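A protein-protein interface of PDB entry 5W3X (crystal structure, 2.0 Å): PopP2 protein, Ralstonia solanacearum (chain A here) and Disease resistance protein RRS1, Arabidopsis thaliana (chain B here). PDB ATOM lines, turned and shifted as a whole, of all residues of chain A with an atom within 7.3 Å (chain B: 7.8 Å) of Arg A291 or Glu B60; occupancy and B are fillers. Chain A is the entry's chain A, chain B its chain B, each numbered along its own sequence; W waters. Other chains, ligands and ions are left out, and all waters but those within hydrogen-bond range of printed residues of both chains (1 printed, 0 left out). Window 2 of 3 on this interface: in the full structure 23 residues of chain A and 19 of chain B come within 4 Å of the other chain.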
ATOM      1  N   ASP A  46       5.885  -7.417  -7.059  1.00  0.00           N
ATOM      2  CA  ASP A  46       7.264  -7.874  -6.980  1.00  0.00           C
ATOM      3  C   ASP A  46       8.217  -6.693  -7.196  1.00  0.00           C
ATOM      4  O   ASP A  46       8.062  -5.941  -8.158  1.00  0.00           O
ATOM      5  CB  ASP A  46       7.525  -8.954  -8.013  1.00  0.00           C
ATOM      6  CG  ASP A  46       8.991  -9.370  -8.063  1.00  0.00           C
ATOM      7  OD1 ASP A  46       9.464  -9.988  -7.086  1.00  0.00           O
ATOM      8  OD2 ASP A  46       9.654  -9.095  -9.084  1.00  0.00           O
ATOM      9  N   GLU A  48      11.415  -6.575  -8.173  1.00  0.00           N
ATOM     10  CA  GLU A  48      12.202  -6.641  -9.399  1.00  0.00           C
ATOM     11  C   GLU A  48      11.388  -6.146 -10.590  1.00  0.00           C
ATOM     12  O   GLU A  48      11.856  -5.311 -11.365  1.00  0.00           O
ATOM     13  CB  GLU A  48      12.696  -8.060  -9.672  1.00  0.00           C
ATOM     14  CG  GLU A  48      13.678  -8.151 -10.856  1.00  0.00           C
ATOM     15  CD  GLU A  48      14.073  -9.591 -11.212  1.00  0.00           C
ATOM     16  OE1 GLU A  48      13.444 -10.535 -10.690  1.00  0.00           O
ATOM     17  OE2 GLU A  48      15.010  -9.775 -12.019  1.00  0.00           O
ATOM     18  N   LEU A  49      10.170  -6.661 -10.734  1.00  0.00           N
ATOM     19  CA  LEU A  49       9.319  -6.265 -11.848  1.00  0.00           C
ATOM     20  C   LEU A  49       8.926  -4.802 -11.741  1.00  0.00           C
ATOM     21  O   LEU A  49       8.749  -4.135 -12.753  1.00  0.00           O
ATOM     22  CB  LEU A  49       8.064  -7.137 -11.915  1.00  0.00           C
ATOM     23  CG  LEU A  49       8.382  -8.586 -12.258  1.00  0.00           C
ATOM     24  CD1 LEU A  49       7.095  -9.372 -12.499  1.00  0.00           C
ATOM     25  CD2 LEU A  49       9.309  -8.637 -13.463  1.00  0.00           C
ATOM     26  N   PHE A 182      16.179 -14.007  -5.581  1.00  0.00           N
ATOM     27  CA  PHE A 182      17.590 -13.697  -5.804  1.00  0.00           C
ATOM     28  C   PHE A 182      18.135 -12.662  -4.816  1.00  0.00           C
ATOM     29  O   PHE A 182      19.343 -12.431  -4.781  1.00  0.00           O
ATOM     30  CB  PHE A 182      17.813 -13.213  -7.243  1.00  0.00           C
ATOM     31  CG  PHE A 182      17.327 -11.799  -7.512  1.00  0.00           C
ATOM     32  CD1 PHE A 182      18.171 -10.711  -7.343  1.00  0.00           C
ATOM     33  CD2 PHE A 182      16.034 -11.570  -7.959  1.00  0.00           C
ATOM     34  CE1 PHE A 182      17.726  -9.421  -7.594  1.00  0.00           C
ATOM     35  CE2 PHE A 182      15.592 -10.287  -8.211  1.00  0.00           C
ATOM     36  CZ  PHE A 182      16.441  -9.213  -8.033  1.00  0.00           C
ATOM     37  N   ARG A 288       1.415 -14.060  -6.923  1.00  0.00           N
ATOM     38  CA  ARG A 288       1.746 -12.939  -7.798  1.00  0.00           C
ATOM     39  C   ARG A 288       2.786 -13.177  -8.868  1.00  0.00           C
ATOM     40  O   ARG A 288       3.431 -14.216  -8.921  1.00  0.00           O
ATOM     41  CB  ARG A 288       2.194 -11.751  -6.964  1.00  0.00           C
ATOM     42  CG  ARG A 288       3.502 -11.873  -6.276  1.00  0.00           C
ATOM     43  CD  ARG A 288       3.628 -10.557  -5.554  1.00  0.00           C
ATOM     44  NE  ARG A 288       4.846 -10.369  -4.830  1.00  0.00           N
ATOM     45  CZ  ARG A 288       4.915  -9.978  -3.565  1.00  0.00           C
ATOM     46  NH1 ARG A 288       3.813  -9.775  -2.848  1.00  0.00           N
ATOM     47  NH2 ARG A 288       6.106  -9.820  -3.016  1.00  0.00           N
ATOM     48  N   LYS A 289       2.909 -12.182  -9.739  1.00  0.00           N
ATOM     49  CA  LYS A 289       3.822 -12.237 -10.861  1.00  0.00           C
ATOM     50  C   LYS A 289       5.238 -11.889 -10.448  1.00  0.00           C
ATOM     51  O   LYS A 289       5.474 -10.892  -9.765  1.00  0.00           O
ATOM     52  CB  LYS A 289       3.366 -11.291 -11.976  1.00  0.00           C
ATOM     53  CG  LYS A 289       2.510 -11.955 -13.029  1.00  0.00           C
ATOM     54  N   VAL A 290       6.174 -12.707 -10.908  1.00  0.00           N
ATOM     55  CA  VAL A 290       7.594 -12.464 -10.728  1.00  0.00           C
ATOM     56  C   VAL A 290       8.252 -12.760 -12.061  1.00  0.00           C
ATOM     57  O   VAL A 290       7.622 -13.363 -12.936  1.00  0.00           O
ATOM     58  CB  VAL A 290       8.204 -13.345  -9.615  1.00  0.00           C
ATOM     59  CG1 VAL A 290       7.622 -12.980  -8.264  1.00  0.00           C
ATOM     60  CG2 VAL A 290       7.995 -14.845  -9.925  1.00  0.00           C
ATOM     61  N   ARG A 291       9.506 -12.344 -12.226  1.00  0.00           N
ATOM     62  CA  ARG A 291      10.238 -12.666 -13.448  1.00  0.00           C
ATOM     63  C   ARG A 291      10.313 -14.171 -13.639  1.00  0.00           C
ATOM     64  O   ARG A 291      10.543 -14.914 -12.683  1.00  0.00           O
ATOM     65  CB  ARG A 291      11.636 -12.062 -13.423  1.00  0.00           C
ATOM     66  CG  ARG A 291      12.613 -12.701 -14.404  1.00  0.00           C
ATOM     67  CD  ARG A 291      13.925 -11.919 -14.443  1.00  0.00           C
ATOM     68  NE  ARG A 291      13.672 -10.506 -14.710  1.00  0.00           N
ATOM     69  CZ  ARG A 291      13.554  -9.990 -15.927  1.00  0.00           C
ATOM     70  NH1 ARG A 291      13.690 -10.766 -16.999  1.00  0.00           N
ATOM     71  NH2 ARG A 291      13.314  -8.696 -16.072  1.00  0.00           N
ATOM     72  N   ASN A 292      10.060 -14.626 -14.861  1.00  0.00           N
ATOM     73  CA  ASN A 292      10.156 -16.041 -15.176  1.00  0.00           C
ATOM     74  C   ASN A 292      11.620 -16.427 -15.062  1.00  0.00           C
ATOM     75  O   ASN A 292      12.482 -15.760 -15.616  1.00  0.00           O
ATOM     76  CB  ASN A 292       9.607 -16.320 -16.581  1.00  0.00           C
ATOM     77  CG  ASN A 292       9.174 -17.771 -16.779  1.00  0.00           C
ATOM     78  OD1 ASN A 292       9.045 -18.541 -15.827  1.00  0.00           O
ATOM     79  ND2 ASN A 292       8.937 -18.143 -18.032  1.00  0.00           N
ATOM     80  N   ARG A 293      11.904 -17.474 -14.305  1.00  0.00           N
ATOM     81  CA  ARG A 293      13.260 -17.961 -14.168  1.00  0.00           C
ATOM     82  C   ARG A 293      13.211 -19.465 -14.314  1.00  0.00           C
ATOM     83  O   ARG A 293      12.166 -20.073 -14.100  1.00  0.00           O
ATOM     84  CB  ARG A 293      13.876 -17.571 -12.817  1.00  0.00           C
ATOM     85  CG  ARG A 293      14.394 -16.151 -12.756  1.00  0.00           C
ATOM     86  CD  ARG A 293      15.144 -15.867 -11.458  1.00  0.00           C
ATOM     87  NE  ARG A 293      15.836 -14.586 -11.558  1.00  0.00           N
ATOM     88  CZ  ARG A 293      15.279 -13.418 -11.254  1.00  0.00           C
ATOM     89  NH1 ARG A 293      14.026 -13.375 -10.804  1.00  0.00           N
ATOM     90  NH2 ARG A 293      15.970 -12.295 -11.395  1.00  0.00           N
ATOM     91  N   ALA A 294      14.337 -20.051 -14.696  1.00  0.00           N
ATOM     92  CA  ALA A 294      14.462 -21.494 -14.801  1.00  0.00           C
ATOM     93  C   ALA A 294      14.193 -22.164 -13.454  1.00  0.00           C
ATOM     94  O   ALA A 294      14.444 -21.577 -12.398  1.00  0.00           O
ATOM     95  CB  ALA A 294      15.839 -21.862 -15.314  1.00  0.00           C
ATOM     96  N   GLY A 303       7.900 -16.115 -22.098  1.00  0.00           N
ATOM     97  CA  GLY A 303       7.305 -14.975 -21.433  1.00  0.00           C
ATOM     98  C   GLY A 303       8.194 -14.518 -20.301  1.00  0.00           C
ATOM     99  O   GLY A 303       8.854 -15.325 -19.644  1.00  0.00           O
ATOM    100  N   GLU A 304       8.204 -13.211 -20.073  1.00  0.00           N
ATOM    101  CA  GLU A 304       9.097 -12.607 -19.100  1.00  0.00           C
ATOM    102  C   GLU A 304       8.665 -12.871 -17.664  1.00  0.00           C
ATOM    103  O   GLU A 304       9.456 -12.688 -16.741  1.00  0.00           O
ATOM    104  CB  GLU A 304       9.203 -11.104 -19.356  1.00  0.00           C
ATOM    105  CG  GLU A 304       9.971 -10.768 -20.625  1.00  0.00           C
ATOM    106  CD  GLU A 304       9.971  -9.288 -20.942  1.00  0.00           C
ATOM    107  OE1 GLU A 304       9.330  -8.518 -20.195  1.00  0.00           O
ATOM    108  OE2 GLU A 304      10.608  -8.895 -21.944  1.00  0.00           O
ATOM    109  N   THR A 305       7.415 -13.290 -17.468  1.00  0.00           N
ATOM    110  CA  THR A 305       6.908 -13.468 -16.113  1.00  0.00           C
ATOM    111  C   THR A 305       6.210 -14.806 -15.884  1.00  0.00           C
ATOM    112  O   THR A 305       5.826 -15.486 -16.830  1.00  0.00           O
ATOM    113  CB  THR A 305       5.911 -12.353 -15.739  1.00  0.00           C
ATOM    114  OG1 THR A 305       4.720 -12.497 -16.522  1.00  0.00           O
ATOM    115  CG2 THR A 305       6.508 -10.975 -15.992  1.00  0.00           C
ATOM    116  N   LYS A 306       6.056 -15.165 -14.611  1.00  0.00           N
ATOM    117  CA  LYS A 306       5.257 -16.323 -14.200  1.00  0.00           C
ATOM    118  C   LYS A 306       4.528 -15.935 -12.923  1.00  0.00           C
ATOM    119  O   LYS A 306       4.989 -15.053 -12.180  1.00  0.00           O
ATOM    120  CB  LYS A 306       6.124 -17.565 -13.965  1.00  0.00           C
ATOM    121  CG  LYS A 306       7.107 -17.407 -12.804  1.00  0.00           C
ATOM    122  CD  LYS A 306       8.039 -18.608 -12.649  1.00  0.00           C
ATOM    123  CE  LYS A 306       9.141 -18.302 -11.635  1.00  0.00           C
ATOM    124  NZ  LYS A 306      10.149 -19.396 -11.539  1.00  0.00           N
ATOM    125  N   ILE A 308       3.324 -17.100  -9.241  1.00  0.00           N
ATOM    126  CA  ILE A 308       3.618 -18.125  -8.254  1.00  0.00           C
ATOM    127  C   ILE A 308       2.900 -17.857  -6.958  1.00  0.00           C
ATOM    128  O   ILE A 308       2.442 -16.744  -6.704  1.00  0.00           O
ATOM    129  CB  ILE A 308       5.119 -18.217  -7.956  1.00  0.00           C
ATOM    130  CG1 ILE A 308       5.626 -16.870  -7.450  1.00  0.00           C
ATOM    131  CG2 ILE A 308       5.877 -18.653  -9.198  1.00  0.00           C
ATOM    132  CD1 ILE A 308       7.062 -16.909  -6.947  1.00  0.00           C
ATOM    133  N   ILE B  30      20.156 -14.326 -10.603  1.00  0.00           N
ATOM    134  CA  ILE B  30      20.746 -13.026 -10.868  1.00  0.00           C
ATOM    135  C   ILE B  30      19.688 -12.011 -11.351  1.00  0.00           C
ATOM    136  O   ILE B  30      18.810 -12.351 -12.154  1.00  0.00           O
ATOM    137  CB  ILE B  30      21.859 -13.147 -11.921  1.00  0.00           C
ATOM    138  CG1 ILE B  30      22.964 -14.074 -11.415  1.00  0.00           C
ATOM    139  CG2 ILE B  30      22.456 -11.776 -12.242  1.00  0.00           C
ATOM    140  CD1 ILE B  30      23.751 -13.487 -10.234  1.00  0.00           C
ATOM    141  N   LEU B  31      19.770 -10.787 -10.829  1.00  0.00           N
ATOM    142  CA  LEU B  31      18.976  -9.654 -11.296  1.00  0.00           C
ATOM    143  C   LEU B  31      18.878  -9.630 -12.810  1.00  0.00           C
ATOM    144  O   LEU B  31      19.893  -9.657 -13.497  1.00  0.00           O
ATOM    145  CB  LEU B  31      19.598  -8.340 -10.817  1.00  0.00           C
ATOM    146  CG  LEU B  31      18.751  -7.093 -10.528  1.00  0.00           C
ATOM    147  CD1 LEU B  31      19.574  -5.811 -10.775  1.00  0.00           C
ATOM    148  CD2 LEU B  31      17.441  -7.059 -11.278  1.00  0.00           C
ATOM    149  N   GLY B  32      17.651  -9.592 -13.320  1.00  0.00           N
ATOM    150  CA  GLY B  32      17.412  -9.376 -14.737  1.00  0.00           C
ATOM    151  C   GLY B  32      17.621 -10.592 -15.624  1.00  0.00           C
ATOM    152  O   GLY B  32      17.466 -10.502 -16.842  1.00  0.00           O
ATOM    153  N   SER B  33      17.958 -11.733 -15.032  1.00  0.00           N
ATOM    154  CA  SER B  33      18.240 -12.919 -15.835  1.00  0.00           C
ATOM    155  C   SER B  33      17.299 -14.076 -15.535  1.00  0.00           C
ATOM    156  O   SER B  33      16.890 -14.287 -14.396  1.00  0.00           O
ATOM    157  CB  SER B  33      19.692 -13.372 -15.633  1.00  0.00           C
ATOM    158  OG  SER B  33      19.984 -14.497 -16.447  1.00  0.00           O
ATOM    159  N   ARG B  34      16.985 -14.846 -16.567  1.00  0.00           N
ATOM    160  CA  ARG B  34      16.137 -16.014 -16.412  1.00  0.00           C
ATOM    161  C   ARG B  34      16.987 -17.189 -15.941  1.00  0.00           C
ATOM    162  O   ARG B  34      16.472 -18.160 -15.392  1.00  0.00           O
ATOM    163  CB  ARG B  34      15.418 -16.339 -17.730  1.00  0.00           C
ATOM    164  CG  ARG B  34      14.238 -15.403 -18.006  1.00  0.00           C
ATOM    165  CD  ARG B  34      13.924 -15.197 -19.477  1.00  0.00           C
ATOM    166  NE  ARG B  34      13.841 -16.435 -20.243  1.00  0.00           N
ATOM    167  CZ  ARG B  34      14.570 -16.680 -21.327  1.00  0.00           C
ATOM    168  NH1 ARG B  34      15.443 -15.778 -21.763  1.00  0.00           N
ATOM    169  NH2 ARG B  34      14.430 -17.827 -21.976  1.00  0.00           N
ATOM    170  N   PHE B  35      18.298 -17.068 -16.112  1.00  0.00           N
ATOM    171  CA  PHE B  35      19.197 -18.175 -15.817  1.00  0.00           C
ATOM    172  C   PHE B  35      20.171 -17.854 -14.687  1.00  0.00           C
ATOM    173  O   PHE B  35      20.720 -16.755 -14.626  1.00  0.00           O
ATOM    174  CB  PHE B  35      19.967 -18.561 -17.075  1.00  0.00           C
ATOM    175  CG  PHE B  35      19.083 -18.899 -18.236  1.00  0.00           C
ATOM    176  CD1 PHE B  35      18.439 -20.122 -18.291  1.00  0.00           C
ATOM    177  CD2 PHE B  35      18.888 -17.994 -19.265  1.00  0.00           C
ATOM    178  CE1 PHE B  35      17.616 -20.445 -19.357  1.00  0.00           C
ATOM    179  CE2 PHE B  35      18.063 -18.307 -20.338  1.00  0.00           C
ATOM    180  CZ  PHE B  35      17.425 -19.534 -20.382  1.00  0.00           C
ATOM    181  N   PRO B  36      20.397 -18.832 -13.797  1.00  0.00           N
ATOM    182  CA  PRO B  36      21.267 -18.662 -12.633  1.00  0.00           C
ATOM    183  C   PRO B  36      22.735 -18.645 -13.018  1.00  0.00           C
ATOM    184  O   PRO B  36      23.107 -19.184 -14.062  1.00  0.00           O
ATOM    185  CB  PRO B  36      20.947 -19.891 -11.780  1.00  0.00           C
ATOM    186  CG  PRO B  36      20.578 -20.922 -12.774  1.00  0.00           C
ATOM    187  CD  PRO B  36      19.828 -20.189 -13.860  1.00  0.00           C
ATOM    188  N   GLN B  57      27.247 -18.788 -16.940  1.00  0.00           N
ATOM    189  CA  GLN B  57      25.855 -18.360 -16.988  1.00  0.00           C
ATOM    190  C   GLN B  57      25.280 -18.454 -18.393  1.00  0.00           C
ATOM    191  O   GLN B  57      25.810 -17.849 -19.324  1.00  0.00           O
ATOM    192  CB  GLN B  57      25.715 -16.931 -16.463  1.00  0.00           C
ATOM    193  CG  GLN B  57      24.274 -16.442 -16.427  1.00  0.00           C
ATOM    194  CD  GLN B  57      24.111 -15.162 -15.641  1.00  0.00           C
ATOM    195  OE1 GLN B  57      25.095 -14.522 -15.262  1.00  0.00           O
ATOM    196  NE2 GLN B  57      22.863 -14.781 -15.386  1.00  0.00           N
ATOM    197  N   ARG B  58      24.196 -19.214 -18.532  1.00  0.00           N
ATOM    198  CA  ARG B  58      23.468 -19.330 -19.794  1.00  0.00           C
ATOM    199  C   ARG B  58      22.936 -17.957 -20.200  1.00  0.00           C
ATOM    200  O   ARG B  58      22.384 -17.232 -19.372  1.00  0.00           O
ATOM    201  CB  ARG B  58      22.338 -20.356 -19.657  1.00  0.00           C
ATOM    202  CG  ARG B  58      21.431 -20.507 -20.875  1.00  0.00           C
ATOM    203  CD  ARG B  58      21.359 -21.964 -21.355  1.00  0.00           C
ATOM    204  NE  ARG B  58      21.382 -22.935 -20.261  1.00  0.00           N
ATOM    205  CZ  ARG B  58      21.706 -24.219 -20.412  1.00  0.00           C
ATOM    206  NH1 ARG B  58      22.062 -24.676 -21.606  1.00  0.00           N
ATOM    207  NH2 ARG B  58      21.698 -25.045 -19.370  1.00  0.00           N
ATOM    208  N   SER B  59      23.135 -17.585 -21.461  1.00  0.00           N
ATOM    209  CA  SER B  59      22.837 -16.225 -21.901  1.00  0.00           C
ATOM    210  C   SER B  59      21.352 -15.902 -21.888  1.00  0.00           C
ATOM    211  O   SER B  59      20.529 -16.685 -22.361  1.00  0.00           O
ATOM    212  CB  SER B  59      23.383 -15.980 -23.305  1.00  0.00           C
ATOM    213  OG  SER B  59      22.989 -14.698 -23.769  1.00  0.00           O
ATOM    214  N   GLU B  60      21.025 -14.735 -21.347  1.00  0.00           N
ATOM    215  CA  GLU B  60      19.647 -14.266 -21.287  1.00  0.00           C
ATOM    216  C   GLU B  60      19.080 -14.078 -22.691  1.00  0.00           C
ATOM    217  O   GLU B  60      18.057 -14.666 -23.041  1.00  0.00           O
ATOM    218  CB  GLU B  60      19.561 -12.957 -20.495  1.00  0.00           C
ATOM    219  CG  GLU B  60      18.205 -12.278 -20.540  1.00  0.00           C
ATOM    220  CD  GLU B  60      17.169 -12.959 -19.663  1.00  0.00           C
ATOM    221  OE1 GLU B  60      17.483 -14.019 -19.080  1.00  0.00           O
ATOM    222  OE2 GLU B  60      16.038 -12.435 -19.561  1.00  0.00           O
ATOM    223  N   THR B  61      19.757 -13.255 -23.487  1.00  0.00           N
ATOM    224  CA  THR B  61      19.290 -12.903 -24.826  1.00  0.00           C
ATOM    225  C   THR B  61      19.209 -14.104 -25.776  1.00  0.00           C
ATOM    226  O   THR B  61      18.176 -14.338 -26.405  1.00  0.00           O
ATOM    227  CB  THR B  61      20.198 -11.826 -25.454  1.00  0.00           C
ATOM    228  OG1 THR B  61      21.554 -12.286 -25.459  1.00  0.00           O
ATOM    229  CG2 THR B  61      20.119 -10.533 -24.653  1.00  0.00           C
ATOM    230  N   ASP B  62      20.295 -14.862 -25.878  1.00  0.00           N
ATOM    231  CA  ASP B  62      20.311 -16.068 -26.700  1.00  0.00           C
ATOM    232  C   ASP B  62      20.455 -17.309 -25.823  1.00  0.00           C
ATOM    233  O   ASP B  62      21.548 -17.617 -25.347  1.00  0.00           O
ATOM    234  CB  ASP B  62      21.448 -16.007 -27.725  1.00  0.00           C
ATOM    235  N   SER B  63      19.353 -18.021 -25.619  1.00  0.00           N
ATOM    236  CA  SER B  63      19.320 -19.173 -24.714  1.00  0.00           C
ATOM    237  C   SER B  63      20.252 -20.317 -25.119  1.00  0.00           C
ATOM    238  O   SER B  63      20.507 -21.232 -24.333  1.00  0.00           O
ATOM    239  CB  SER B  63      17.889 -19.702 -24.604  1.00  0.00           C
ATOM    240  OG  SER B  63      17.867 -20.975 -23.982  1.00  0.00           O
ATOM    241  N   ASN B  64      20.753 -20.265 -26.348  1.00  0.00           N
ATOM    242  CA  ASN B  64      21.634 -21.307 -26.859  1.00  0.00           C
ATOM    243  C   ASN B  64      23.093 -21.063 -26.466  1.00  0.00           C
ATOM    244  O   ASN B  64      23.904 -21.990 -26.417  1.00  0.00           O
ATOM    245  CB  ASN B  64      21.499 -21.405 -28.384  1.00  0.00           C
ATOM    246  N   MET B  65      23.412 -19.808 -26.167  1.00  0.00           N
ATOM    247  CA  MET B  65      24.769 -19.398 -25.829  1.00  0.00           C
ATOM    248  C   MET B  65      25.098 -19.493 -24.333  1.00  0.00           C
ATOM    249  O   MET B  65      24.272 -19.156 -23.483  1.00  0.00           O
ATOM    250  CB  MET B  65      25.005 -17.965 -26.313  1.00  0.00           C
ATOM    251  N   ALA B  67      27.764 -18.116 -21.431  1.00  0.00           N
ATOM    252  CA  ALA B  67      28.788 -17.123 -21.129  1.00  0.00           C
ATOM    253  C   ALA B  67      29.687 -17.638 -20.010  1.00  0.00           C
ATOM    254  O   ALA B  67      29.212 -18.080 -18.961  1.00  0.00           O
ATOM    255  CB  ALA B  67      28.157 -15.796 -20.739  1.00  0.00           C
HETATM  256  O   HOH W   1      18.324 -15.827 -12.441  1.00  0.00           O
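The backbone NH of Gly B32 lies within hydrogen-bond range of the side-chain carboxylate of Glu A48 (2.9 Å).
The guanidinium group (NH1) of Arg A291 is in salt-bridge range of the side-chain carboxylate (OE2) of Glu B60 (3.9 Å).
The guanidinium group of Arg A293 lies within hydrogen-bond range of the backbone carbonyl oxygen of Ile B30, 2.9 Å away.
The guanidinium group (NE) of Arg A293 sits at hydrogen-bond distance from the backbone carbonyl oxygen (O) of Ser B33, at 3.0 Å.
The backbone NH of Ala A294 lies within hydrogen-bond range of the backbone carbonyl oxygen of Arg B34 (2.9 Å).
OD2 of Asp A46 sits at hydrogen-bond distance from N of Glu A48.
The guanidinium group (NE) of Arg A291 is in salt-bridge range of the side-chain carboxylate (OE2) of Glu A48, 3.1 Å away.
OE2 of Glu A48 is in salt-bridge range of NH2 of Arg A293 (2.8 Å).
ND2 of Asn A292 lies within hydrogen-bond range of O of Gly A303, at 3.2 Å.
O of Arg A293 lies within hydrogen-bond range of NZ of Lys A306 (3.3 Å).
O of Phe B35 lies within hydrogen-bond range of OG of Ser B33, 3.0 Å away.
Among the printed residues, pairs that only touch across the chains: Asn A292 with Arg B34, Arg A293 with Arg B34, Glu A48 with Leu B31, Arg A293 with Gly B32, Arg A291 with Gly B32, Arg A291 with Ser B33 and Phe A182 with Leu B31.
Of the printed residues of chain A, Ile B30 touches Arg A293 (2.9 Å).
Of the printed residues of chain B, Glu A48 touches Leu B31 (3.7 Å) and Gly B32 (2.9 Å).
Printed residues of chain A within 4 Å of Gly B32: Glu A48 (2.9 Å), Arg A291 (3.8 Å) and Arg A293 (3.7 Å).
Printed residues of chain A within 4 Å of Leu B31: Glu A48 and Phe A182.
The nearest residue of chain B that does not touch Arg A291 is Arg B34 (4.7 Å).
Of the 17 printed residues of chain B, 6 touch a printed residue of chain A.
Hydrophobic or aromatic side chains of chain A within 4 Å of the printed part of chain B: Phe A182 and Ala A294.
Water W1 lies within hydrogen-bond range of the backbone carbonyl oxygen of Ser B33, the guanidinium group of Arg A293, the backbone NH of Ile B30 and the backbone carbonyl oxygen of Phe B35.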
